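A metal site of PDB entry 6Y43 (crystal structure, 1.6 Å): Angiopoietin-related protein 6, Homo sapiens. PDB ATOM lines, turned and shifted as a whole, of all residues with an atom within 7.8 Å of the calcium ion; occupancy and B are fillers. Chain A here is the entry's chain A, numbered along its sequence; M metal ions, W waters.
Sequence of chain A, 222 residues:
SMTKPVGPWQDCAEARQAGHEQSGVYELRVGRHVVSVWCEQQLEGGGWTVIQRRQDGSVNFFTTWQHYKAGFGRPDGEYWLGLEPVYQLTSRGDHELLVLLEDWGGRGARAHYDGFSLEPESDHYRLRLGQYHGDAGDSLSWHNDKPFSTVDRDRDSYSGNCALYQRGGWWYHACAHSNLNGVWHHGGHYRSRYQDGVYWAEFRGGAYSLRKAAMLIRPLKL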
ATOM      1  N   SER A 149      13.182 -14.172 -13.492  1.00  0.00           N
ATOM      2  CA  SER A 149      12.124 -15.032 -13.991  1.00  0.00           C
ATOM      3  C   SER A 149      10.835 -14.263 -14.239  1.00  0.00           C
ATOM      4  O   SER A 149      10.472 -13.347 -13.467  1.00  0.00           O
ATOM      5  CB  SER A 149      11.791 -16.183 -13.005  1.00  0.00           C
ATOM      6  OG  SER A 149      12.786 -17.169 -12.930  1.00  0.00           O
ATOM      7  N   ARG A 153       9.175 -17.816 -18.271  1.00  0.00           N
ATOM      8  CA  ARG A 153      10.618 -18.012 -18.173  1.00  0.00           C
ATOM      9  C   ARG A 153      10.914 -18.367 -16.723  1.00  0.00           C
ATOM     10  O   ARG A 153      11.387 -17.546 -15.941  1.00  0.00           O
ATOM     11  CB  ARG A 153      11.361 -16.795 -18.626  1.00  0.00           C
ATOM     12  CG  ARG A 153      11.525 -16.718 -20.155  1.00  0.00           C
ATOM     13  CD  ARG A 153      11.835 -15.315 -20.463  1.00  0.00           C
ATOM     14  NE  ARG A 153      12.157 -14.978 -21.848  1.00  0.00           N
ATOM     15  CZ  ARG A 153      11.259 -14.827 -22.816  1.00  0.00           C
ATOM     16  NH1 ARG A 153       9.979 -15.095 -22.613  1.00  0.00           N
ATOM     17  NH2 ARG A 153      11.663 -14.416 -24.005  1.00  0.00           N
ATOM     18  N   ASP A 154      10.610 -19.608 -16.376  1.00  0.00           N
ATOM     19  CA  ASP A 154      10.844 -20.135 -15.032  1.00  0.00           C
ATOM     20  C   ASP A 154      12.310 -20.509 -14.907  1.00  0.00           C
ATOM     21  O   ASP A 154      12.749 -21.561 -15.384  1.00  0.00           O
ATOM     22  CB  ASP A 154       9.938 -21.335 -14.757  1.00  0.00           C
ATOM     23  CG  ASP A 154      10.156 -21.965 -13.385  1.00  0.00           C
ATOM     24  OD1 ASP A 154      11.128 -21.595 -12.687  1.00  0.00           O
ATOM     25  OD2 ASP A 154       9.350 -22.849 -13.023  1.00  0.00           O
ATOM     26  N   ARG A 155      13.077 -19.632 -14.271  1.00  0.00           N
ATOM     27  CA  ARG A 155      14.501 -19.823 -14.019  1.00  0.00           C
ATOM     28  C   ARG A 155      14.797 -19.946 -12.539  1.00  0.00           C
ATOM     29  O   ARG A 155      15.950 -19.842 -12.124  1.00  0.00           O
ATOM     30  CB  ARG A 155      15.287 -18.662 -14.603  1.00  0.00           C
ATOM     31  CG  ARG A 155      15.069 -18.556 -16.059  1.00  0.00           C
ATOM     32  CD  ARG A 155      15.389 -17.191 -16.596  1.00  0.00           C
ATOM     33  NE  ARG A 155      15.477 -17.292 -18.043  1.00  0.00           N
ATOM     34  CZ  ARG A 155      15.379 -16.272 -18.871  1.00  0.00           C
ATOM     35  NH1 ARG A 155      15.190 -15.048 -18.384  1.00  0.00           N
ATOM     36  NH2 ARG A 155      15.483 -16.480 -20.175  1.00  0.00           N
ATOM     37  N   ASP A 156      13.756 -20.098 -11.730  1.00  0.00           N
ATOM     38  CA  ASP A 156      13.939 -20.016 -10.294  1.00  0.00           C
ATOM     39  C   ASP A 156      14.448 -21.363  -9.758  1.00  0.00           C
ATOM     40  O   ASP A 156      14.758 -22.303 -10.491  1.00  0.00           O
ATOM     41  CB  ASP A 156      12.628 -19.582  -9.630  1.00  0.00           C
ATOM     42  CG  ASP A 156      11.492 -20.568  -9.813  1.00  0.00           C
ATOM     43  OD1 ASP A 156      11.713 -21.803  -9.696  1.00  0.00           O
ATOM     44  OD2 ASP A 156      10.341 -20.115 -10.018  1.00  0.00           O
ATOM     45  N   SER A 157      14.570 -21.414  -8.439  1.00  0.00           N
ATOM     46  CA  SER A 157      15.086 -22.603  -7.760  1.00  0.00           C
ATOM     47  C   SER A 157      13.986 -23.382  -7.046  1.00  0.00           C
ATOM     48  O   SER A 157      14.260 -24.157  -6.144  1.00  0.00           O
ATOM     49  CB  SER A 157      16.172 -22.181  -6.777  1.00  0.00           C
ATOM     50  OG  SER A 157      17.289 -21.653  -7.484  1.00  0.00           O
ATOM     51  N   TYR A 158      12.743 -23.197  -7.487  1.00  0.00           N
ATOM     52  CA  TYR A 158      11.562 -23.814  -6.931  1.00  0.00           C
ATOM     53  C   TYR A 158      11.052 -24.924  -7.840  1.00  0.00           C
ATOM     54  O   TYR A 158      11.202 -24.891  -9.045  1.00  0.00           O
ATOM     55  CB  TYR A 158      10.463 -22.769  -6.729  1.00  0.00           C
ATOM     56  CG  TYR A 158       9.210 -23.260  -6.072  1.00  0.00           C
ATOM     57  CD1 TYR A 158       9.254 -24.010  -4.902  1.00  0.00           C
ATOM     58  CD2 TYR A 158       7.974 -22.962  -6.616  1.00  0.00           C
ATOM     59  CE1 TYR A 158       8.088 -24.449  -4.291  1.00  0.00           C
ATOM     60  CE2 TYR A 158       6.801 -23.373  -6.013  1.00  0.00           C
ATOM     61  CZ  TYR A 158       6.869 -24.140  -4.849  1.00  0.00           C
ATOM     62  OH  TYR A 158       5.696 -24.559  -4.275  1.00  0.00           O
ATOM     63  N   SER A 159      10.465 -25.948  -7.215  1.00  0.00           N
ATOM     64  CA  SER A 159       9.912 -27.076  -7.952  1.00  0.00           C
ATOM     65  C   SER A 159       8.835 -26.639  -8.922  1.00  0.00           C
ATOM     66  O   SER A 159       8.650 -27.244  -9.965  1.00  0.00           O
ATOM     67  CB  SER A 159       9.298 -28.137  -7.005  1.00  0.00           C
ATOM     68  OG  SER A 159       9.980 -28.289  -5.794  1.00  0.00           O
ATOM     69  N   GLY A 160       8.097 -25.628  -8.552  1.00  0.00           N
ATOM     70  CA  GLY A 160       7.092 -25.056  -9.404  1.00  0.00           C
ATOM     71  C   GLY A 160       7.485 -23.734  -9.931  1.00  0.00           C
ATOM     72  O   GLY A 160       8.673 -23.420 -10.000  1.00  0.00           O
ATOM     73  N   ASN A 161       6.540 -22.949 -10.325  1.00  0.00           N
ATOM     74  CA  ASN A 161       6.757 -21.693 -11.048  1.00  0.00           C
ATOM     75  C   ASN A 161       6.444 -20.527 -10.107  1.00  0.00           C
ATOM     76  O   ASN A 161       5.286 -20.135  -9.942  1.00  0.00           O
ATOM     77  CB  ASN A 161       5.873 -21.655 -12.295  1.00  0.00           C
ATOM     78  CG  ASN A 161       6.180 -20.455 -13.191  1.00  0.00           C
ATOM     79  OD1 ASN A 161       6.624 -19.398 -12.733  1.00  0.00           O
ATOM     80  ND2 ASN A 161       5.881 -20.596 -14.464  1.00  0.00           N
ATOM     81  N   CYS A 162       7.493 -19.951  -9.508  1.00  0.00           N
ATOM     82  CA  CYS A 162       7.264 -18.909  -8.514  1.00  0.00           C
ATOM     83  C   CYS A 162       6.447 -17.750  -9.065  1.00  0.00           C
ATOM     84  O   CYS A 162       5.523 -17.251  -8.405  1.00  0.00           O
ATOM     85  CB  CYS A 162       8.587 -18.378  -7.981  1.00  0.00           C
ATOM     86  SG  CYS A 162       9.494 -19.546  -6.994  1.00  0.00           S
ATOM     87  N   ALA A 163       6.758 -17.309 -10.292  1.00  0.00           N
ATOM     88  CA  ALA A 163       6.064 -16.160 -10.874  1.00  0.00           C
ATOM     89  C   ALA A 163       4.576 -16.429 -11.071  1.00  0.00           C
ATOM     90  O   ALA A 163       3.755 -15.518 -10.993  1.00  0.00           O
ATOM     91  CB  ALA A 163       6.709 -15.827 -12.222  1.00  0.00           C
ATOM     92  N   TYR A 172      13.424 -14.684  -8.543  1.00  0.00           N
ATOM     93  CA  TYR A 172      12.860 -15.653  -7.612  1.00  0.00           C
ATOM     94  C   TYR A 172      13.871 -16.742  -7.261  1.00  0.00           C
ATOM     95  O   TYR A 172      14.659 -17.207  -8.103  1.00  0.00           O
ATOM     96  CB  TYR A 172      11.567 -16.282  -8.181  1.00  0.00           C
ATOM     97  CG  TYR A 172      10.352 -15.341  -8.177  1.00  0.00           C
ATOM     98  CD1 TYR A 172       9.822 -14.844  -6.985  1.00  0.00           C
ATOM     99  CD2 TYR A 172       9.737 -14.974  -9.364  1.00  0.00           C
ATOM    100  CE1 TYR A 172       8.730 -13.994  -7.000  1.00  0.00           C
ATOM    101  CE2 TYR A 172       8.646 -14.133  -9.376  1.00  0.00           C
ATOM    102  CZ  TYR A 172       8.124 -13.662  -8.168  1.00  0.00           C
ATOM    103  OH  TYR A 172       7.029 -12.803  -8.185  1.00  0.00           O
ATOM    104  N   HIS A 173      13.815 -17.158  -5.984  1.00  0.00           N
ATOM    105  CA  HIS A 173      14.624 -18.231  -5.425  1.00  0.00           C
ATOM    106  C   HIS A 173      13.684 -19.392  -5.211  1.00  0.00           C
ATOM    107  O   HIS A 173      13.296 -20.073  -6.189  1.00  0.00           O
ATOM    108  CB  HIS A 173      15.287 -17.737  -4.132  1.00  0.00           C
ATOM    109  CG  HIS A 173      16.310 -18.668  -3.565  1.00  0.00           C
ATOM    110  ND1 HIS A 173      17.409 -18.224  -2.869  1.00  0.00           N
ATOM    111  CD2 HIS A 173      16.396 -20.020  -3.558  1.00  0.00           C
ATOM    112  CE1 HIS A 173      18.142 -19.255  -2.476  1.00  0.00           C
ATOM    113  NE2 HIS A 173      17.539 -20.360  -2.886  1.00  0.00           N
ATOM    114  N   CYS A 175      10.492 -19.392  -2.617  1.00  0.00           N
ATOM    115  CA  CYS A 175      10.399 -18.514  -3.779  1.00  0.00           C
ATOM    116  C   CYS A 175      10.935 -17.125  -3.518  1.00  0.00           C
ATOM    117  O   CYS A 175      11.637 -16.549  -4.375  1.00  0.00           O
ATOM    118  CB  CYS A 175       8.954 -18.350  -4.231  1.00  0.00           C
ATOM    119  SG  CYS A 175       8.396 -19.736  -5.249  1.00  0.00           S
HETATM  120 CA    CA M   1      10.733 -23.424 -10.994  1.00  0.00          CA
HETATM  121  O   HOH W   1      13.006 -24.035 -11.474  1.00  0.00           O
HETATM  122  O   HOH W   2      10.193 -25.594 -11.974  1.00  0.00           O
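The side-chain sulfur (SG) of Cys 162 forms a disulfide with the side-chain sulfur (SG) of Cys 175 (2.1 Å). The backbone carbonyl oxygen (O) of His 173 is in hydrogen-bond range of the backbone NH (N) of Tyr 158, 3.4 Å away. The backbone NH of Cys 162 lies within hydrogen-bond range of the side-chain carboxylate of Asp 156, 2.9 Å away. The backbone NH (N) of Asp 156 is in hydrogen-bond range of the side-chain hydroxyl (OG) of Ser 149, at 3.3 Å.
Of the 15 residues printed, 4 come within 4 Å of the calcium ion.
O of Gly 160 is bound to the calcium ion. The side-chain carboxylate (OD1) of Asp 156 is bound to the calcium ion (2.3 Å). Water W1 binds the calcium ion (2.4 Å). The calcium ion is bound by water W2 (2.4 Å). O of Tyr 158 is bound to the calcium ion (2.5 Å). The calcium ion is bound by OD2 of Asp 154 (2.5 Å). OD1 of Asp 154 is bound to the calcium ion, at 2.5 Å. The calcium ion has seven donor atoms within binding distance.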
